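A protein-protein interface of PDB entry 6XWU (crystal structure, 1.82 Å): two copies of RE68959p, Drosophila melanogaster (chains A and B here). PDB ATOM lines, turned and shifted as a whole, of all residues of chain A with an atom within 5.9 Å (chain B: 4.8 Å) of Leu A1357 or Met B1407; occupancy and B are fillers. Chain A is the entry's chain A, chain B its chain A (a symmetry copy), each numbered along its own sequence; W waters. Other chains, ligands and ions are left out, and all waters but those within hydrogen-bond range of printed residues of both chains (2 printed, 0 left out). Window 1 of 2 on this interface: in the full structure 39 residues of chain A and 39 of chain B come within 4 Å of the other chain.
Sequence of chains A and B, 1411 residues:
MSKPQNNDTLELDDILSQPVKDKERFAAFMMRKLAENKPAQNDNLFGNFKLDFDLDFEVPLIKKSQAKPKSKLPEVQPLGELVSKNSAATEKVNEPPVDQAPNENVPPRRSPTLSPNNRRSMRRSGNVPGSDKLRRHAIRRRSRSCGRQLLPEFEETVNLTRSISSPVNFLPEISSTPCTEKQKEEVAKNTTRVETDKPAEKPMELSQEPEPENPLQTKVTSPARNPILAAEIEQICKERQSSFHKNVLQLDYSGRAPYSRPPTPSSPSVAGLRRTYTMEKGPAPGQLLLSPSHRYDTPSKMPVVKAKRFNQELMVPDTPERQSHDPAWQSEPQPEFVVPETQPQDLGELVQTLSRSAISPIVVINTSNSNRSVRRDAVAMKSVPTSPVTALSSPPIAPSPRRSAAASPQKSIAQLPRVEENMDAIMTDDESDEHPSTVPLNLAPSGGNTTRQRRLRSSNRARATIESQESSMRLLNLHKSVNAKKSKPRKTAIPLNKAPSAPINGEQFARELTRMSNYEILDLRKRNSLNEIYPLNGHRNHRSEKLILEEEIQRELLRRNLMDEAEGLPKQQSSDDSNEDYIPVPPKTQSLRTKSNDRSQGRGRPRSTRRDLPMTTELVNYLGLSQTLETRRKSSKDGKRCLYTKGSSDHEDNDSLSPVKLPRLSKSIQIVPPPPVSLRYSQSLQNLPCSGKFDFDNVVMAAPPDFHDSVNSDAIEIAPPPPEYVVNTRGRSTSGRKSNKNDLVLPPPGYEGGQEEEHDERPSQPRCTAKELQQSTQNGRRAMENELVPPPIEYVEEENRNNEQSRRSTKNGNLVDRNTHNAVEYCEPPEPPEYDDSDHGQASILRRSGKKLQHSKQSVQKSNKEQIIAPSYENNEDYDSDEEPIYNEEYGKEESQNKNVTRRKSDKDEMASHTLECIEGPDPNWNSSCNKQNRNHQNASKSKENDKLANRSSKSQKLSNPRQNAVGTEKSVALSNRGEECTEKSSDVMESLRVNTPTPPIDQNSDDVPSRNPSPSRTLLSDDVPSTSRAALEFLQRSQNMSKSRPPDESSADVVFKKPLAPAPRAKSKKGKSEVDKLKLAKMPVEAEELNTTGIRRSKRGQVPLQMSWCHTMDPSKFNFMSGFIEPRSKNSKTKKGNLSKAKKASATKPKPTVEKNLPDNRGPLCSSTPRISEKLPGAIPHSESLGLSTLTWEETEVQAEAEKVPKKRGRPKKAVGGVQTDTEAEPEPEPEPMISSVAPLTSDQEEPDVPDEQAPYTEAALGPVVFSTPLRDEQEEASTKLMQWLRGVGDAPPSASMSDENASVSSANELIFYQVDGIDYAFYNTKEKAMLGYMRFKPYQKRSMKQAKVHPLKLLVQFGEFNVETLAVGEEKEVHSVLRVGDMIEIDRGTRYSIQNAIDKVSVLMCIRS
NE2 of Gln A1359 lies close to NE2 of Gln B1359 (3.2 Å).
O of Gly A1383 is in hydrogen-bond range of OH of Tyr B1325 (2.6 Å).
Of the 14 printed residues of chain A, 7 touch a printed residue of chain B.
Hydrophobic or aromatic side chains of chain B within 4 Å of the printed part of chain A: Tyr B1325, Leu B1333, Leu B1357, Met B1407 and Ile B1409.
Among the printed residues, no Asp or Glu carboxylate lies within 4 Å of a Lys or Arg side-chain nitrogen of the other chain.
Of chain A, only Leu A1357 comes within 4 Å of Met B1407.
Of the printed residues of chain A, Tyr B1325 touches Leu A1357 (3.3 Å), Gly A1383 (2.6 Å) and Met A1385 (3.6 Å).
Printed residues of chain B within 4 Å of Ile A1409: Leu B1333 (3.7 Å) and Ile B1409 (3.7 Å).
Of the printed residues of chain B, Met A1407 touches Leu B1357 (3.6 Å).
The nearest residue of chain A that does not touch Met B1407 is Met A1407 (4.1 Å).
The nearest printed residue of chain A that does not touch Ile B1409 is Met A1407 (4.9 Å).
Leu A1357 touches Met B1407, and with the chains exchanged Met A1407 touches Leu B1357.
Gln B1359 touches its own counterpart, Gln A1359.
Ile B1409 touches its own counterpart, Ile A1409.
Positions printed for both chains: 1355, 1356, 1357, 1359, 1405, 1406, 1407, 1408 and 1409.
Of the 10 pairs that touch across the chains among the printed residues, 4 have their exchanged pair printed and touching as well.
Water W1 bridges NE2 of Gln A1359 (2.9 Å) and NE2 of Gln B1359 (3.1 Å).
Water W2 lies within hydrogen-bond range of the side-chain amide nitrogen of Gln B1359, the side-chain amide nitrogen of Gln A1359 and the side-chain hydroxyl of Tyr B1335.
Among the printed residues, pairs that only touch across the chains: Lys A1355 with Leu B1333 (3.9 Å), Leu A1357 with Tyr B1325 (3.3 Å), Leu A1357 with Met B1407 (3.6 Å), Met A1385 with Tyr B1325 (3.6 Å), Met A1385 with Leu B1333 (3.8 Å), Met A1407 with Leu B1357 (3.6 Å), Ile A1409 with Leu B1333 (3.7 Å) and Ile A1409 with Ile B1409 (3.7 Å).
O of Ile A1409 lies within hydrogen-bond range of N of Lys A1355 (2.7 Å).
The backbone carbonyl oxygen of Leu A1357 lies within hydrogen-bond range of the backbone NH of Met A1407, 2.7 Å away.
The backbone NH (N) of Gln A1359 lies within hydrogen-bond range of the backbone carbonyl oxygen (O) of Val A1405.
O of Leu B1333 sits at hydrogen-bond distance from N of Tyr B1325, at 3.0 Å.
OH of Tyr B1325 sits at hydrogen-bond distance from OH of Tyr B1335 (2.8 Å).
The backbone carbonyl oxygen of Ile B1409 is in hydrogen-bond range of the backbone NH of Lys B1355, 2.7 Å away.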
ATOM      1  N   LYS A1355      29.415  10.722  17.384  1.00  0.00           N
ATOM      2  CA  LYS A1355      28.602   9.926  16.486  1.00  0.00           C
ATOM      3  C   LYS A1355      27.600   9.164  17.332  1.00  0.00           C
ATOM      4  O   LYS A1355      27.934   8.692  18.419  1.00  0.00           O
ATOM      5  CB  LYS A1355      29.461   8.961  15.648  1.00  0.00           C
ATOM      6  CG  LYS A1355      30.530   9.666  14.798  1.00  0.00           C
ATOM      7  CD  LYS A1355      31.456   8.670  14.109  1.00  0.00           C
ATOM      8  CE  LYS A1355      32.603   9.377  13.402  1.00  0.00           C
ATOM      9  NZ  LYS A1355      33.550   9.971  14.377  1.00  0.00           N
ATOM     10  N   LEU A1356      26.370   9.080  16.855  1.00  0.00           N
ATOM     11  CA  LEU A1356      25.330   8.300  17.517  1.00  0.00           C
ATOM     12  C   LEU A1356      24.961   7.163  16.588  1.00  0.00           C
ATOM     13  O   LEU A1356      24.642   7.406  15.422  1.00  0.00           O
ATOM     14  CB  LEU A1356      24.097   9.152  17.826  1.00  0.00           C
ATOM     15  CG  LEU A1356      24.358  10.453  18.579  1.00  0.00           C
ATOM     16  CD1 LEU A1356      23.063  11.267  18.637  1.00  0.00           C
ATOM     17  CD2 LEU A1356      24.879  10.160  19.970  1.00  0.00           C
ATOM     18  N   LEU A1357      25.033   5.927  17.089  1.00  0.00           N
ATOM     19  CA  LEU A1357      24.841   4.740  16.264  1.00  0.00           C
ATOM     20  C   LEU A1357      23.755   3.896  16.922  1.00  0.00           C
ATOM     21  O   LEU A1357      23.875   3.550  18.100  1.00  0.00           O
ATOM     22  CB  LEU A1357      26.152   3.959  16.138  1.00  0.00           C
ATOM     23  CG  LEU A1357      26.175   2.640  15.360  1.00  0.00           C
ATOM     24  CD1 LEU A1357      25.511   2.810  14.018  1.00  0.00           C
ATOM     25  CD2 LEU A1357      27.606   2.185  15.175  1.00  0.00           C
ATOM     26  N   VAL A1358      22.696   3.582  16.183  1.00  0.00           N
ATOM     27  CA  VAL A1358      21.540   2.915  16.781  1.00  0.00           C
ATOM     28  C   VAL A1358      21.848   1.435  16.969  1.00  0.00           C
ATOM     29  O   VAL A1358      22.183   0.729  16.011  1.00  0.00           O
ATOM     30  CB  VAL A1358      20.275   3.107  15.932  1.00  0.00           C
ATOM     31  CG1 VAL A1358      19.090   2.421  16.609  1.00  0.00           C
ATOM     32  CG2 VAL A1358      19.980   4.596  15.740  1.00  0.00           C
ATOM     33  N   GLN A1359      21.739   0.966  18.215  1.00  0.00           N
ATOM     34  CA  GLN A1359      21.967  -0.439  18.543  1.00  0.00           C
ATOM     35  C   GLN A1359      20.676  -1.234  18.594  1.00  0.00           C
ATOM     36  O   GLN A1359      20.677  -2.431  18.284  1.00  0.00           O
ATOM     37  CB  GLN A1359      22.698  -0.548  19.880  1.00  0.00           C
ATOM     38  CG  GLN A1359      24.184  -0.276  19.758  1.00  0.00           C
ATOM     39  CD  GLN A1359      24.970  -1.560  19.589  1.00  0.00           C
ATOM     40  OE1 GLN A1359      24.680  -2.562  20.238  1.00  0.00           O
ATOM     41  NE2 GLN A1359      25.960  -1.542  18.705  1.00  0.00           N
ATOM     42  N   GLY A1383      21.653   0.265  13.230  1.00  0.00           N
ATOM     43  CA  GLY A1383      22.789   0.345  12.324  1.00  0.00           C
ATOM     44  C   GLY A1383      22.991   1.689  11.642  1.00  0.00           C
ATOM     45  O   GLY A1383      24.047   1.898  11.022  1.00  0.00           O
ATOM     46  N   ASP A1384      22.015   2.594  11.707  1.00  0.00           N
ATOM     47  CA  ASP A1384      22.189   3.944  11.177  1.00  0.00           C
ATOM     48  C   ASP A1384      23.006   4.786  12.153  1.00  0.00           C
ATOM     49  O   ASP A1384      22.920   4.628  13.376  1.00  0.00           O
ATOM     50  CB  ASP A1384      20.832   4.622  10.943  1.00  0.00           C
ATOM     51  CG  ASP A1384      19.999   3.949   9.868  1.00  0.00           C
ATOM     52  OD1 ASP A1384      20.526   3.124   9.074  1.00  0.00           O
ATOM     53  OD2 ASP A1384      18.781   4.252   9.820  1.00  0.00           O
ATOM     54  N   MET A1385      23.775   5.722  11.610  1.00  0.00           N
ATOM     55  CA  MET A1385      24.616   6.595  12.414  1.00  0.00           C
ATOM     56  C   MET A1385      24.381   8.050  12.012  1.00  0.00           C
ATOM     57  O   MET A1385      24.065   8.342  10.855  1.00  0.00           O
ATOM     58  CB  MET A1385      26.097   6.222  12.219  1.00  0.00           C
ATOM     59  CG  MET A1385      27.048   6.995  13.092  1.00  0.00           C
ATOM     60  SD  MET A1385      27.802   8.293  12.111  1.00  0.00           S
ATOM     61  CE  MET A1385      28.736   7.254  11.046  1.00  0.00           C
ATOM     62  N   ILE A1386      24.507   8.962  12.970  1.00  0.00           N
ATOM     63  CA  ILE A1386      24.502  10.392  12.666  1.00  0.00           C
ATOM     64  C   ILE A1386      25.729  11.016  13.317  1.00  0.00           C
ATOM     65  O   ILE A1386      26.106  10.658  14.442  1.00  0.00           O
ATOM     66  CB  ILE A1386      23.194  11.092  13.117  1.00  0.00           C
ATOM     67  CG1 ILE A1386      23.148  12.553  12.638  1.00  0.00           C
ATOM     68  CG2 ILE A1386      23.009  11.030  14.648  1.00  0.00           C
ATOM     69  CD1 ILE A1386      21.755  13.192  12.714  1.00  0.00           C
ATOM     70  N   VAL A1405      18.002   1.754  22.184  1.00  0.00           N
ATOM     71  CA  VAL A1405      19.380   1.845  22.670  1.00  0.00           C
ATOM     72  C   VAL A1405      20.238   2.476  21.583  1.00  0.00           C
ATOM     73  O   VAL A1405      20.189   2.053  20.419  1.00  0.00           O
ATOM     74  CB  VAL A1405      19.952   0.463  23.045  1.00  0.00           C
ATOM     75  CG1 VAL A1405      21.383   0.598  23.550  1.00  0.00           C
ATOM     76  CG2 VAL A1405      19.069  -0.246  24.087  1.00  0.00           C
ATOM     77  N   LEU A1406      21.058   3.456  21.954  1.00  0.00           N
ATOM     78  CA  LEU A1406      22.017   3.970  20.988  1.00  0.00           C
ATOM     79  C   LEU A1406      23.414   3.967  21.595  1.00  0.00           C
ATOM     80  O   LEU A1406      23.584   4.029  22.813  1.00  0.00           O
ATOM     81  CB  LEU A1406      21.634   5.371  20.473  1.00  0.00           C
ATOM     82  CG  LEU A1406      21.666   6.645  21.303  1.00  0.00           C
ATOM     83  CD1 LEU A1406      23.080   7.103  21.608  1.00  0.00           C
ATOM     84  CD2 LEU A1406      20.933   7.756  20.555  1.00  0.00           C
ATOM     85  N   MET A1407      24.407   3.855  20.725  1.00  0.00           N
ATOM     86  CA  MET A1407      25.804   3.933  21.113  1.00  0.00           C
ATOM     87  C   MET A1407      26.275   5.363  20.881  1.00  0.00           C
ATOM     88  O   MET A1407      25.962   5.968  19.849  1.00  0.00           O
ATOM     89  CB  MET A1407      26.635   2.934  20.304  1.00  0.00           C
ATOM     90  CG  MET A1407      28.120   2.994  20.603  1.00  0.00           C
ATOM     91  SD  MET A1407      29.141   1.869  19.628  1.00  0.00           S
ATOM     92  CE  MET A1407      28.316   0.299  19.888  1.00  0.00           C
ATOM     93  N   CYS A1408      26.982   5.913  21.863  1.00  0.00           N
ATOM     94  CA  CYS A1408      27.531   7.261  21.792  1.00  0.00           C
ATOM     95  C   CYS A1408      29.042   7.154  21.661  1.00  0.00           C
ATOM     96  O   CYS A1408      29.691   6.559  22.529  1.00  0.00           O
ATOM     97  CB  CYS A1408      27.155   8.069  23.031  1.00  0.00           C
ATOM     98  SG  CYS A1408      27.849   9.722  23.009  1.00  0.00           S
ATOM     99  N   ILE A1409      29.588   7.723  20.578  1.00  0.00           N
ATOM    100  CA  ILE A1409      31.013   7.675  20.247  1.00  0.00           C
ATOM    101  C   ILE A1409      31.519   9.105  20.209  1.00  0.00           C
ATOM    102  O   ILE A1409      31.194   9.848  19.276  1.00  0.00           O
ATOM    103  CB  ILE A1409      31.269   7.002  18.888  1.00  0.00           C
ATOM    104  CG1 ILE A1409      30.596   5.628  18.790  1.00  0.00           C
ATOM    105  CG2 ILE A1409      32.753   6.955  18.581  1.00  0.00           C
ATOM    106  CD1 ILE A1409      30.619   5.047  17.383  1.00  0.00           C
ATOM    107  N   TYR B1325      31.238   3.434   7.279  1.00  0.00           N
ATOM    108  CA  TYR B1325      30.295   4.528   7.090  1.00  0.00           C
ATOM    109  C   TYR B1325      30.971   5.677   6.349  1.00  0.00           C
ATOM    110  O   TYR B1325      32.186   5.865   6.434  1.00  0.00           O
ATOM    111  CB  TYR B1325      29.784   5.030   8.432  1.00  0.00           C
ATOM    112  CG  TYR B1325      28.922   4.035   9.191  1.00  0.00           C
ATOM    113  CD1 TYR B1325      27.569   3.886   8.889  1.00  0.00           C
ATOM    114  CD2 TYR B1325      29.460   3.256  10.215  1.00  0.00           C
ATOM    115  CE1 TYR B1325      26.773   2.963   9.581  1.00  0.00           C
ATOM    116  CE2 TYR B1325      28.660   2.334  10.914  1.00  0.00           C
ATOM    117  CZ  TYR B1325      27.324   2.203  10.594  1.00  0.00           C
ATOM    118  OH  TYR B1325      26.532   1.293  11.281  1.00  0.00           O
ATOM    119  N   LEU B1333      34.896   4.961  11.077  1.00  0.00           N
ATOM    120  CA  LEU B1333      33.956   4.073  11.763  1.00  0.00           C
ATOM    121  C   LEU B1333      33.486   3.007  10.790  1.00  0.00           C
ATOM    122  O   LEU B1333      32.905   3.332   9.751  1.00  0.00           O
ATOM    123  CB  LEU B1333      32.761   4.862  12.314  1.00  0.00           C
ATOM    124  CG  LEU B1333      31.730   4.069  13.104  1.00  0.00           C
ATOM    125  CD1 LEU B1333      32.348   3.572  14.407  1.00  0.00           C
ATOM    126  CD2 LEU B1333      30.519   4.934  13.399  1.00  0.00           C
ATOM    127  N   GLY B1334      33.707   1.744  11.125  1.00  0.00           N
ATOM    128  CA  GLY B1334      33.332   0.690  10.205  1.00  0.00           C
ATOM    129  C   GLY B1334      33.406  -0.669  10.859  1.00  0.00           C
ATOM    130  O   GLY B1334      33.558  -0.787  12.078  1.00  0.00           O
ATOM    131  N   TYR B1335      33.282  -1.696  10.022  1.00  0.00           N
ATOM    132  CA  TYR B1335      33.263  -3.081  10.466  1.00  0.00           C
ATOM    133  C   TYR B1335      34.327  -3.878   9.723  1.00  0.00           C
ATOM    134  O   TYR B1335      34.600  -3.626   8.549  1.00  0.00           O
ATOM    135  CB  TYR B1335      31.886  -3.739  10.213  1.00  0.00           C
ATOM    136  CG  TYR B1335      30.740  -2.998  10.852  1.00  0.00           C
ATOM    137  CD1 TYR B1335      30.352  -3.282  12.153  1.00  0.00           C
ATOM    138  CD2 TYR B1335      30.050  -2.007  10.155  1.00  0.00           C
ATOM    139  CE1 TYR B1335      29.309  -2.602  12.763  1.00  0.00           C
ATOM    140  CE2 TYR B1335      28.993  -1.316  10.755  1.00  0.00           C
ATOM    141  CZ  TYR B1335      28.621  -1.629  12.050  1.00  0.00           C
ATOM    142  OH  TYR B1335      27.600  -0.941  12.664  1.00  0.00           O
ATOM    143  N   LYS B1355      39.673   1.933  18.730  1.00  0.00           N
ATOM    144  CA  LYS B1355      38.999   0.988  19.598  1.00  0.00           C
ATOM    145  C   LYS B1355      38.417  -0.104  18.720  1.00  0.00           C
ATOM    146  O   LYS B1355      37.917   0.175  17.630  1.00  0.00           O
ATOM    147  CB  LYS B1355      37.897   1.669  20.432  1.00  0.00           C
ATOM    148  CG  LYS B1355      38.412   2.818  21.313  1.00  0.00           C
ATOM    149  CD  LYS B1355      37.273   3.563  21.998  1.00  0.00           C
ATOM    150  CE  LYS B1355      37.779   4.792  22.738  1.00  0.00           C
ATOM    151  NZ  LYS B1355      38.235   5.839  21.792  1.00  0.00           N
ATOM    152  N   LEU B1356      38.517  -1.341  19.174  1.00  0.00           N
ATOM    153  CA  LEU B1356      37.920  -2.477  18.479  1.00  0.00           C
ATOM    154  C   LEU B1356      36.839  -3.036  19.379  1.00  0.00           C
ATOM    155  O   LEU B1356      37.109  -3.337  20.544  1.00  0.00           O
ATOM    156  CB  LEU B1356      38.960  -3.555  18.166  1.00  0.00           C
ATOM    157  CG  LEU B1356      40.217  -3.080  17.444  1.00  0.00           C
ATOM    158  CD1 LEU B1356      41.224  -4.231  17.380  1.00  0.00           C
ATOM    159  CD2 LEU B1356      39.870  -2.583  16.056  1.00  0.00           C
ATOM    160  N   LEU B1357      35.616  -3.148  18.854  1.00  0.00           N
ATOM    161  CA  LEU B1357      34.460  -3.538  19.652  1.00  0.00           C
ATOM    162  C   LEU B1357      33.807  -4.730  18.960  1.00  0.00           C
ATOM    163  O   LEU B1357      33.467  -4.641  17.777  1.00  0.00           O
ATOM    164  CB  LEU B1357      33.481  -2.368  19.785  1.00  0.00           C
ATOM    165  CG  LEU B1357      32.163  -2.566  20.537  1.00  0.00           C
ATOM    166  CD1 LEU B1357      32.411  -3.222  21.870  1.00  0.00           C
ATOM    167  CD2 LEU B1357      31.487  -1.227  20.737  1.00  0.00           C
ATOM    168  N   GLN B1359      31.250  -7.151  17.574  1.00  0.00           N
ATOM    169  CA  GLN B1359      29.832  -7.138  17.222  1.00  0.00           C
ATOM    170  C   GLN B1359      29.250  -8.535  17.133  1.00  0.00           C
ATOM    171  O   GLN B1359      28.062  -8.727  17.419  1.00  0.00           O
ATOM    172  CB  GLN B1359      29.633  -6.406  15.895  1.00  0.00           C
ATOM    173  CG  GLN B1359      29.668  -4.899  16.048  1.00  0.00           C
ATOM    174  CD  GLN B1359      28.274  -4.326  16.205  1.00  0.00           C
ATOM    175  OE1 GLN B1359      27.341  -4.755  15.531  1.00  0.00           O
ATOM    176  NE2 GLN B1359      28.122  -3.362  17.106  1.00  0.00           N
ATOM    177  N   VAL B1405      32.679 -10.640  13.558  1.00  0.00           N
ATOM    178  CA  VAL B1405      32.562  -9.255  13.097  1.00  0.00           C
ATOM    179  C   VAL B1405      33.033  -8.330  14.211  1.00  0.00           C
ATOM    180  O   VAL B1405      32.603  -8.468  15.366  1.00  0.00           O
ATOM    181  CB  VAL B1405      31.114  -8.898  12.705  1.00  0.00           C
ATOM    182  CG1 VAL B1405      31.033  -7.453  12.227  1.00  0.00           C
ATOM    183  CG2 VAL B1405      30.570  -9.859  11.634  1.00  0.00           C
ATOM    184  N   LEU B1406      33.880  -7.361  13.874  1.00  0.00           N
ATOM    185  CA  LEU B1406      34.220  -6.353  14.867  1.00  0.00           C
ATOM    186  C   LEU B1406      34.010  -4.961  14.283  1.00  0.00           C
ATOM    187  O   LEU B1406      34.065  -4.760  13.070  1.00  0.00           O
ATOM    188  CB  LEU B1406      35.655  -6.523  15.403  1.00  0.00           C
ATOM    189  CG  LEU B1406      36.922  -6.277  14.599  1.00  0.00           C
ATOM    190  CD1 LEU B1406      37.159  -4.803  14.327  1.00  0.00           C
ATOM    191  CD2 LEU B1406      38.121  -6.843  15.357  1.00  0.00           C
ATOM    192  N   MET B1407      33.730  -4.016  15.168  1.00  0.00           N
ATOM    193  CA  MET B1407      33.596  -2.617  14.806  1.00  0.00           C
ATOM    194  C   MET B1407      34.930  -1.933  15.074  1.00  0.00           C
ATOM    195  O   MET B1407      35.559  -2.169  16.112  1.00  0.00           O
ATOM    196  CB  MET B1407      32.465  -1.967  15.608  1.00  0.00           C
ATOM    197  CG  MET B1407      32.298  -0.485  15.336  1.00  0.00           C
ATOM    198  SD  MET B1407      31.011   0.329  16.305  1.00  0.00           S
ATOM    199  CE  MET B1407      29.594  -0.725  16.000  1.00  0.00           C
ATOM    200  N   CYS B1408      35.380  -1.129  14.115  1.00  0.00           N
ATOM    201  CA  CYS B1408      36.624  -0.379  14.223  1.00  0.00           C
ATOM    202  C   CYS B1408      36.281   1.094  14.377  1.00  0.00           C
ATOM    203  O   CYS B1408      35.606   1.659  13.509  1.00  0.00           O
ATOM    204  CB  CYS B1408      37.502  -0.599  12.993  1.00  0.00           C
ATOM    205  SG  CYS B1408      39.026   0.342  13.060  1.00  0.00           S
ATOM    206  N   ILE B1409      36.738   1.701  15.480  1.00  0.00           N
ATOM    207  CA  ILE B1409      36.463   3.093  15.835  1.00  0.00           C
ATOM    208  C   ILE B1409      37.796   3.815  15.910  1.00  0.00           C
ATOM    209  O   ILE B1409      38.565   3.592  16.851  1.00  0.00           O
ATOM    210  CB  ILE B1409      35.736   3.214  17.184  1.00  0.00           C
ATOM    211  CG1 ILE B1409      34.482   2.334  17.243  1.00  0.00           C
ATOM    212  CG2 ILE B1409      35.452   4.666  17.515  1.00  0.00           C
ATOM    213  CD1 ILE B1409      33.881   2.238  18.638  1.00  0.00           C
HETATM  214  O   HOH W   1      27.642  -3.411  20.178  1.00  0.00           O
HETATM  215  O   HOH W   2      26.040  -1.963  15.625  1.00  0.00           O
